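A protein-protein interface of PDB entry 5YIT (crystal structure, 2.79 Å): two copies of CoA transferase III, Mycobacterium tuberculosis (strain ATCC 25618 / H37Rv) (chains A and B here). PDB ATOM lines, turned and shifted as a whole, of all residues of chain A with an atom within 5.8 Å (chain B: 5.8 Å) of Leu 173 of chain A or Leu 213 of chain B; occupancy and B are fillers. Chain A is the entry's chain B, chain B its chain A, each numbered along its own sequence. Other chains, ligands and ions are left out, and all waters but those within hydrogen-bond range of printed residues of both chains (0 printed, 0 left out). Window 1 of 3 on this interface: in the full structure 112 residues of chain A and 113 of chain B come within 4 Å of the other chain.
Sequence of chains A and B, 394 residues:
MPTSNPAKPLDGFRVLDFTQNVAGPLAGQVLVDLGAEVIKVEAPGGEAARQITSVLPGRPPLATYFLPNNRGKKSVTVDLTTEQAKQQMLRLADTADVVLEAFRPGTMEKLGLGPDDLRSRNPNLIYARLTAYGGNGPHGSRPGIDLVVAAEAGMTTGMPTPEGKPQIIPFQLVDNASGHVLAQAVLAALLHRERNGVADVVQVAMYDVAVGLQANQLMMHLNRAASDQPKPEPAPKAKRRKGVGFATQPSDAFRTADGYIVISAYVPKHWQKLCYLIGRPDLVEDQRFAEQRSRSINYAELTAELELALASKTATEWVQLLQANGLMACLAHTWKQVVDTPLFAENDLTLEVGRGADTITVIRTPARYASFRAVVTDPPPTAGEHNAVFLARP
Printed residues of chain B that touch a printed residue of chain A: Met 155, Ile 169, Phe 171, Leu 173, Ala 177, Gly 212, Leu 213 and Asn 216. Hydrophobic or aromatic side chains of chain B within 4 Å of the printed part of chain A: Met 155, Ile 169, Phe 171, Leu 173 and Leu 213. Among the printed residues, 15 pairs touch across the chains.
ND2 of Asn 176 of chain A sits at hydrogen-bond distance from O of Gln 172 of chain A.
The backbone carbonyl oxygen of Leu 213 of chain B sits at hydrogen-bond distance from the side-chain amide nitrogen of Asn 176 of chain A (3.4 Å). OD1 of Asn 216 of chain B sits at hydrogen-bond distance from ND2 of Asn 176 of chain A, 3.2 Å away.
Met 155 of chain A touches Phe 171 of chain B (O to CE2, 3.8 Å). CD1 of Ile 169 of chain A touches CD1 of Ile 169 of chain B (3.9 Å). Phe 171 of chain A touches Leu 213 of chain B. Gln 172 of chain A touches Asn 216 of chain B (NE2 to OD1, 3.5 Å). Leu 173 of chain B touches Leu 173 of chain A. Leu 173 of chain A touches Leu 213 of chain B (O to CD2, 3.8 Å). CG of Asn 176 of chain A touches O of Gly 212 of chain B, 3.8 Å away. N of Ala 177 of chain A touches CD2 of Leu 213 of chain B, 3.9 Å away. Phe 171 of chain B touches Leu 213 of chain A. Leu 213 of chain A touches Leu 173 of chain B (CD2 to O, 3.9 Å).
Of the printed residues of chain B, Ile 169 of chain A touches Ile 169 (3.9 Å). Leu 173 of chain A touches two residues of chain B. Printed residues of chain A within 4 Å of Phe 171 of chain B: Met 155 and Leu 213. Printed residues of chain A within 4 Å of Leu 173 of chain B: Leu 173 and Leu 213. Printed residues of chain A within 4 Å of Ala 177 of chain B: Leu 213. Val 211 of chain B touches none of the printed residues of chain A. Of chain A, only Phe 171, Gln 172, Leu 173, Asn 176 and Ala 177 come within 4 Å of Leu 213 of chain B. The nearest printed residue of chain A that does not touch Leu 213 of chain B is Val 174 of chain A (5.8 Å).
Met 155 of chain A touches Phe 171 of chain B, and with the chains exchanged Phe 171 of chain A touches Met 155 of chain B. Phe 171 of chain A touches Leu 213 of chain B, and with the chains exchanged Leu 213 of chain A touches Phe 171 of chain B. Leu 173 of chain A touches its own counterpart, Leu 173 of chain B. Leu 173 of chain A touches Leu 213 of chain B, and with the chains exchanged Leu 213 of chain A touches Leu 173 of chain B. Of the 15 pairs that touch across the chains among the printed residues, 10 have their exchanged pair printed and touching as well.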
ATOM      1  N   ASP A 146      -8.227 -15.301 -12.869  1.00  0.00           N
ATOM      2  CA  ASP A 146      -8.122 -14.594 -11.602  1.00  0.00           C
ATOM      3  C   ASP A 146      -9.000 -13.349 -11.486  1.00  0.00           C
ATOM      4  O   ASP A 146      -9.717 -13.169 -10.482  1.00  0.00           O
ATOM      5  CB  ASP A 146      -6.680 -14.216 -11.321  1.00  0.00           C
ATOM      6  CG  ASP A 146      -6.502 -13.583  -9.950  1.00  0.00           C
ATOM      7  OD1 ASP A 146      -6.634 -12.334  -9.895  1.00  0.00           O
ATOM      8  OD2 ASP A 146      -6.196 -14.329  -8.959  1.00  0.00           O
ATOM      9  N   MET A 155     -14.789  -8.912  -4.723  1.00  0.00           N
ATOM     10  CA  MET A 155     -13.535  -8.359  -4.213  1.00  0.00           C
ATOM     11  C   MET A 155     -13.348  -6.871  -4.506  1.00  0.00           C
ATOM     12  O   MET A 155     -12.454  -6.247  -3.964  1.00  0.00           O
ATOM     13  CB  MET A 155     -12.343  -9.183  -4.663  1.00  0.00           C
ATOM     14  CG  MET A 155     -12.287 -10.539  -4.009  1.00  0.00           C
ATOM     15  SD  MET A 155     -10.742 -11.426  -4.300  1.00  0.00           S
ATOM     16  CE  MET A 155     -10.694 -12.582  -2.925  1.00  0.00           C
ATOM     17  N   ILE A 169      -7.843  -5.295  -8.332  1.00  0.00           N
ATOM     18  CA  ILE A 169      -6.595  -5.525  -7.701  1.00  0.00           C
ATOM     19  C   ILE A 169      -5.607  -6.049  -8.720  1.00  0.00           C
ATOM     20  O   ILE A 169      -5.883  -6.959  -9.445  1.00  0.00           O
ATOM     21  CB  ILE A 169      -6.770  -6.526  -6.577  1.00  0.00           C
ATOM     22  CG1 ILE A 169      -7.975  -6.143  -5.707  1.00  0.00           C
ATOM     23  CG2 ILE A 169      -5.555  -6.546  -5.686  1.00  0.00           C
ATOM     24  CD1 ILE A 169      -7.964  -6.766  -4.318  1.00  0.00           C
ATOM     25  N   PHE A 171      -2.861  -7.698  -8.535  1.00  0.00           N
ATOM     26  CA  PHE A 171      -2.084  -8.927  -8.396  1.00  0.00           C
ATOM     27  C   PHE A 171      -2.990 -10.097  -8.342  1.00  0.00           C
ATOM     28  O   PHE A 171      -4.141  -9.953  -8.010  1.00  0.00           O
ATOM     29  CB  PHE A 171      -1.116  -8.933  -7.220  1.00  0.00           C
ATOM     30  CG  PHE A 171      -1.716  -8.523  -5.939  1.00  0.00           C
ATOM     31  CD1 PHE A 171      -1.914  -7.181  -5.652  1.00  0.00           C
ATOM     32  CD2 PHE A 171      -2.030  -9.469  -4.997  1.00  0.00           C
ATOM     33  CE1 PHE A 171      -2.429  -6.809  -4.451  1.00  0.00           C
ATOM     34  CE2 PHE A 171      -2.562  -9.101  -3.785  1.00  0.00           C
ATOM     35  CZ  PHE A 171      -2.761  -7.769  -3.504  1.00  0.00           C
ATOM     36  N   GLN A 172      -2.449 -11.265  -8.656  1.00  0.00           N
ATOM     37  CA  GLN A 172      -3.251 -12.468  -8.756  1.00  0.00           C
ATOM     38  C   GLN A 172      -3.470 -13.134  -7.416  1.00  0.00           C
ATOM     39  O   GLN A 172      -2.980 -14.218  -7.172  1.00  0.00           O
ATOM     40  CB  GLN A 172      -2.592 -13.434  -9.711  1.00  0.00           C
ATOM     41  CG  GLN A 172      -2.679 -13.035 -11.168  1.00  0.00           C
ATOM     42  CD  GLN A 172      -1.927 -11.763 -11.444  1.00  0.00           C
ATOM     43  OE1 GLN A 172      -2.451 -10.873 -12.086  1.00  0.00           O
ATOM     44  NE2 GLN A 172      -0.715 -11.645 -10.899  1.00  0.00           N
ATOM     45  N   LEU A 173      -4.244 -12.482  -6.565  1.00  0.00           N
ATOM     46  CA  LEU A 173      -4.504 -12.930  -5.224  1.00  0.00           C
ATOM     47  C   LEU A 173      -5.310 -14.249  -5.162  1.00  0.00           C
ATOM     48  O   LEU A 173      -5.025 -15.111  -4.358  1.00  0.00           O
ATOM     49  CB  LEU A 173      -5.184 -11.788  -4.498  1.00  0.00           C
ATOM     50  CG  LEU A 173      -6.353 -11.973  -3.572  1.00  0.00           C
ATOM     51  CD1 LEU A 173      -5.920 -12.335  -2.156  1.00  0.00           C
ATOM     52  CD2 LEU A 173      -7.115 -10.671  -3.565  1.00  0.00           C
ATOM     53  N   VAL A 174      -6.297 -14.408  -6.024  1.00  0.00           N
ATOM     54  CA  VAL A 174      -7.070 -15.619  -6.029  1.00  0.00           C
ATOM     55  C   VAL A 174      -6.299 -16.795  -6.600  1.00  0.00           C
ATOM     56  O   VAL A 174      -6.372 -17.888  -6.073  1.00  0.00           O
ATOM     57  CB  VAL A 174      -8.332 -15.448  -6.864  1.00  0.00           C
ATOM     58  CG1 VAL A 174      -9.055 -16.771  -7.020  1.00  0.00           C
ATOM     59  CG2 VAL A 174      -9.226 -14.394  -6.249  1.00  0.00           C
ATOM     60  N   ASP A 175      -5.571 -16.579  -7.679  1.00  0.00           N
ATOM     61  CA  ASP A 175      -4.799 -17.653  -8.286  1.00  0.00           C
ATOM     62  C   ASP A 175      -3.766 -18.127  -7.327  1.00  0.00           C
ATOM     63  O   ASP A 175      -3.542 -19.305  -7.192  1.00  0.00           O
ATOM     64  CB  ASP A 175      -4.000 -17.147  -9.462  1.00  0.00           C
ATOM     65  CG  ASP A 175      -4.715 -17.231 -10.756  1.00  0.00           C
ATOM     66  OD1 ASP A 175      -5.900 -17.519 -10.746  1.00  0.00           O
ATOM     67  OD2 ASP A 175      -4.098 -16.979 -11.801  1.00  0.00           O
ATOM     68  N   ASN A 176      -3.090 -17.187  -6.690  1.00  0.00           N
ATOM     69  CA  ASN A 176      -2.046 -17.547  -5.773  1.00  0.00           C
ATOM     70  C   ASN A 176      -2.557 -18.187  -4.505  1.00  0.00           C
ATOM     71  O   ASN A 176      -1.969 -19.141  -4.016  1.00  0.00           O
ATOM     72  CB  ASN A 176      -1.111 -16.376  -5.495  1.00  0.00           C
ATOM     73  CG  ASN A 176      -0.081 -16.196  -6.599  1.00  0.00           C
ATOM     74  OD1 ASN A 176       0.769 -17.055  -6.810  1.00  0.00           O
ATOM     75  ND2 ASN A 176      -0.166 -15.101  -7.317  1.00  0.00           N
ATOM     76  N   ALA A 177      -3.673 -17.702  -3.981  1.00  0.00           N
ATOM     77  CA  ALA A 177      -4.210 -18.304  -2.778  1.00  0.00           C
ATOM     78  C   ALA A 177      -4.783 -19.663  -3.098  1.00  0.00           C
ATOM     79  O   ALA A 177      -4.627 -20.566  -2.325  1.00  0.00           O
ATOM     80  CB  ALA A 177      -5.252 -17.430  -2.162  1.00  0.00           C
ATOM     81  N   SER A 178      -5.423 -19.801  -4.248  1.00  0.00           N
ATOM     82  CA  SER A 178      -5.979 -21.067  -4.605  1.00  0.00           C
ATOM     83  C   SER A 178      -4.916 -22.120  -4.772  1.00  0.00           C
ATOM     84  O   SER A 178      -5.151 -23.288  -4.470  1.00  0.00           O
ATOM     85  CB  SER A 178      -6.722 -20.957  -5.892  1.00  0.00           C
ATOM     86  OG  SER A 178      -7.772 -20.035  -5.741  1.00  0.00           O
ATOM     87  N   LEU A 213     -11.477 -15.717   1.519  1.00  0.00           N
ATOM     88  CA  LEU A 213     -10.626 -14.591   1.847  1.00  0.00           C
ATOM     89  C   LEU A 213     -11.433 -13.378   2.322  1.00  0.00           C
ATOM     90  O   LEU A 213     -10.888 -12.541   3.053  1.00  0.00           O
ATOM     91  CB  LEU A 213      -9.802 -14.184   0.631  1.00  0.00           C
ATOM     92  CG  LEU A 213      -8.840 -15.248   0.087  1.00  0.00           C
ATOM     93  CD1 LEU A 213      -8.386 -14.875  -1.311  1.00  0.00           C
ATOM     94  CD2 LEU A 213      -7.624 -15.445   0.981  1.00  0.00           C
ATOM     95  N   MET B 155       0.809  -4.037  -1.182  1.00  0.00           N
ATOM     96  CA  MET B 155      -0.489  -4.396  -1.745  1.00  0.00           C
ATOM     97  C   MET B 155      -1.304  -3.173  -2.183  1.00  0.00           C
ATOM     98  O   MET B 155      -2.381  -3.303  -2.787  1.00  0.00           O
ATOM     99  CB  MET B 155      -1.278  -5.280  -0.777  1.00  0.00           C
ATOM    100  CG  MET B 155      -0.649  -6.654  -0.592  1.00  0.00           C
ATOM    101  SD  MET B 155      -1.711  -7.845   0.278  1.00  0.00           S
ATOM    102  CE  MET B 155      -0.903  -9.391  -0.186  1.00  0.00           C
ATOM    103  N   ILE B 169      -7.151  -2.486   0.837  1.00  0.00           N
ATOM    104  CA  ILE B 169      -8.091  -3.585   0.605  1.00  0.00           C
ATOM    105  C   ILE B 169      -8.917  -3.868   1.876  1.00  0.00           C
ATOM    106  O   ILE B 169      -8.370  -4.223   2.918  1.00  0.00           O
ATOM    107  CB  ILE B 169      -7.400  -4.869   0.113  1.00  0.00           C
ATOM    108  CG1 ILE B 169      -6.649  -4.596  -1.196  1.00  0.00           C
ATOM    109  CG2 ILE B 169      -8.416  -6.018   0.008  1.00  0.00           C
ATOM    110  CD1 ILE B 169      -5.594  -5.649  -1.492  1.00  0.00           C
ATOM    111  N   PHE B 171     -10.848  -6.119   2.980  1.00  0.00           N
ATOM    112  CA  PHE B 171     -10.967  -7.419   3.573  1.00  0.00           C
ATOM    113  C   PHE B 171      -9.597  -7.970   4.015  1.00  0.00           C
ATOM    114  O   PHE B 171      -8.552  -7.559   3.508  1.00  0.00           O
ATOM    115  CB  PHE B 171     -11.726  -8.389   2.660  1.00  0.00           C
ATOM    116  CG  PHE B 171     -11.093  -8.625   1.312  1.00  0.00           C
ATOM    117  CD1 PHE B 171     -10.126  -9.609   1.125  1.00  0.00           C
ATOM    118  CD2 PHE B 171     -11.542  -7.920   0.202  1.00  0.00           C
ATOM    119  CE1 PHE B 171      -9.615  -9.878  -0.150  1.00  0.00           C
ATOM    120  CE2 PHE B 171     -11.000  -8.149  -1.073  1.00  0.00           C
ATOM    121  CZ  PHE B 171     -10.037  -9.139  -1.247  1.00  0.00           C
ATOM    122  N   LEU B 173      -7.280 -10.254   3.485  1.00  0.00           N
ATOM    123  CA  LEU B 173      -6.690 -11.268   2.574  1.00  0.00           C
ATOM    124  C   LEU B 173      -5.429 -11.931   3.163  1.00  0.00           C
ATOM    125  O   LEU B 173      -5.279 -13.140   3.100  1.00  0.00           O
ATOM    126  CB  LEU B 173      -6.389 -10.693   1.173  1.00  0.00           C
ATOM    127  CG  LEU B 173      -5.301  -9.607   1.070  1.00  0.00           C
ATOM    128  CD1 LEU B 173      -4.820  -9.527  -0.346  1.00  0.00           C
ATOM    129  CD2 LEU B 173      -5.771  -8.241   1.580  1.00  0.00           C
ATOM    130  N   VAL B 174      -4.547 -11.138   3.743  1.00  0.00           N
ATOM    131  CA  VAL B 174      -3.301 -11.649   4.287  1.00  0.00           C
ATOM    132  C   VAL B 174      -3.576 -12.639   5.409  1.00  0.00           C
ATOM    133  O   VAL B 174      -2.928 -13.707   5.468  1.00  0.00           O
ATOM    134  CB  VAL B 174      -2.375 -10.511   4.814  1.00  0.00           C
ATOM    135  CG1 VAL B 174      -1.079 -11.070   5.392  1.00  0.00           C
ATOM    136  CG2 VAL B 174      -2.106  -9.485   3.716  1.00  0.00           C
ATOM    137  N   ALA B 177      -5.206 -15.950   3.850  1.00  0.00           N
ATOM    138  CA  ALA B 177      -4.193 -16.627   3.032  1.00  0.00           C
ATOM    139  C   ALA B 177      -3.154 -17.254   3.949  1.00  0.00           C
ATOM    140  O   ALA B 177      -2.787 -18.399   3.754  1.00  0.00           O
ATOM    141  CB  ALA B 177      -3.548 -15.700   2.017  1.00  0.00           C
ATOM    142  N   ASP B 208       5.722 -12.930   4.430  1.00  0.00           N
ATOM    143  CA  ASP B 208       6.186 -13.810   3.355  1.00  0.00           C
ATOM    144  C   ASP B 208       5.033 -14.303   2.510  1.00  0.00           C
ATOM    145  O   ASP B 208       5.164 -14.379   1.280  1.00  0.00           O
ATOM    146  CB  ASP B 208       6.991 -14.973   3.891  1.00  0.00           C
ATOM    147  CG  ASP B 208       8.258 -14.535   4.627  1.00  0.00           C
ATOM    148  OD1 ASP B 208       8.500 -13.328   4.880  1.00  0.00           O
ATOM    149  OD2 ASP B 208       9.042 -15.445   4.955  1.00  0.00           O
ATOM    150  N   VAL B 209       3.904 -14.590   3.167  1.00  0.00           N
ATOM    151  CA  VAL B 209       2.675 -15.007   2.481  1.00  0.00           C
ATOM    152  C   VAL B 209       2.205 -13.897   1.534  1.00  0.00           C
ATOM    153  O   VAL B 209       1.856 -14.164   0.374  1.00  0.00           O
ATOM    154  CB  VAL B 209       1.532 -15.331   3.506  1.00  0.00           C
ATOM    155  CG1 VAL B 209       0.157 -15.446   2.832  1.00  0.00           C
ATOM    156  CG2 VAL B 209       1.850 -16.550   4.350  1.00  0.00           C
ATOM    157  N   ALA B 210       2.180 -12.677   2.068  1.00  0.00           N
ATOM    158  CA  ALA B 210       1.735 -11.517   1.334  1.00  0.00           C
ATOM    159  C   ALA B 210       2.630 -11.272   0.112  1.00  0.00           C
ATOM    160  O   ALA B 210       2.132 -10.888  -0.969  1.00  0.00           O
ATOM    161  CB  ALA B 210       1.721 -10.292   2.246  1.00  0.00           C
ATOM    162  N   VAL B 211       3.937 -11.469   0.297  1.00  0.00           N
ATOM    163  CA  VAL B 211       4.888 -11.296  -0.768  1.00  0.00           C
ATOM    164  C   VAL B 211       4.570 -12.332  -1.860  1.00  0.00           C
ATOM    165  O   VAL B 211       4.615 -12.033  -3.069  1.00  0.00           O
ATOM    166  CB  VAL B 211       6.350 -11.444  -0.261  1.00  0.00           C
ATOM    167  CG1 VAL B 211       7.286 -11.840  -1.396  1.00  0.00           C
ATOM    168  CG2 VAL B 211       6.826 -10.181   0.412  1.00  0.00           C
ATOM    169  N   GLY B 212       4.269 -13.550  -1.433  1.00  0.00           N
ATOM    170  CA  GLY B 212       3.946 -14.613  -2.379  1.00  0.00           C
ATOM    171  C   GLY B 212       2.698 -14.337  -3.187  1.00  0.00           C
ATOM    172  O   GLY B 212       2.648 -14.736  -4.354  1.00  0.00           O
ATOM    173  N   LEU B 213       1.702 -13.672  -2.582  1.00  0.00           N
ATOM    174  CA  LEU B 213       0.480 -13.323  -3.287  1.00  0.00           C
ATOM    175  C   LEU B 213       0.732 -12.349  -4.430  1.00  0.00           C
ATOM    176  O   LEU B 213      -0.015 -12.332  -5.419  1.00  0.00           O
ATOM    177  CB  LEU B 213      -0.570 -12.757  -2.343  1.00  0.00           C
ATOM    178  CG  LEU B 213      -1.161 -13.753  -1.345  1.00  0.00           C
ATOM    179  CD1 LEU B 213      -1.991 -13.017  -0.319  1.00  0.00           C
ATOM    180  CD2 LEU B 213      -2.039 -14.748  -2.078  1.00  0.00           C
ATOM    181  N   GLN B 214       1.768 -11.551  -4.316  1.00  0.00           N
ATOM    182  CA  GLN B 214       2.109 -10.589  -5.337  1.00  0.00           C
ATOM    183  C   GLN B 214       3.367 -10.954  -6.049  1.00  0.00           C
ATOM    184  O   GLN B 214       3.972 -10.127  -6.629  1.00  0.00           O
ATOM    185  CB  GLN B 214       2.276  -9.214  -4.734  1.00  0.00           C
ATOM    186  CG  GLN B 214       1.634  -9.012  -3.391  1.00  0.00           C
ATOM    187  CD  GLN B 214       1.922  -7.662  -2.832  1.00  0.00           C
ATOM    188  OE1 GLN B 214       1.602  -6.681  -3.422  1.00  0.00           O
ATOM    189  NE2 GLN B 214       2.540  -7.618  -1.695  1.00  0.00           N
ATOM    190  N   ALA B 215       3.740 -12.208  -6.039  1.00  0.00           N
ATOM    191  CA  ALA B 215       4.990 -12.633  -6.601  1.00  0.00           C
ATOM    192  C   ALA B 215       5.192 -12.364  -8.025  1.00  0.00           C
ATOM    193  O   ALA B 215       6.282 -12.068  -8.402  1.00  0.00           O
ATOM    194  CB  ALA B 215       5.184 -14.093  -6.358  1.00  0.00           C
ATOM    195  N   ASN B 216       4.178 -12.520  -8.844  1.00  0.00           N
ATOM    196  CA  ASN B 216       4.338 -12.237 -10.255  1.00  0.00           C
ATOM    197  C   ASN B 216       4.652 -10.800 -10.491  1.00  0.00           C
ATOM    198  O   ASN B 216       5.415 -10.489 -11.345  1.00  0.00           O
ATOM    199  CB  ASN B 216       3.093 -12.592 -11.007  1.00  0.00           C
ATOM    200  CG  ASN B 216       2.448 -13.820 -10.468  1.00  0.00           C
ATOM    201  OD1 ASN B 216       1.750 -13.762  -9.476  1.00  0.00           O
ATOM    202  ND2 ASN B 216       2.686 -14.944 -11.113  1.00  0.00           N
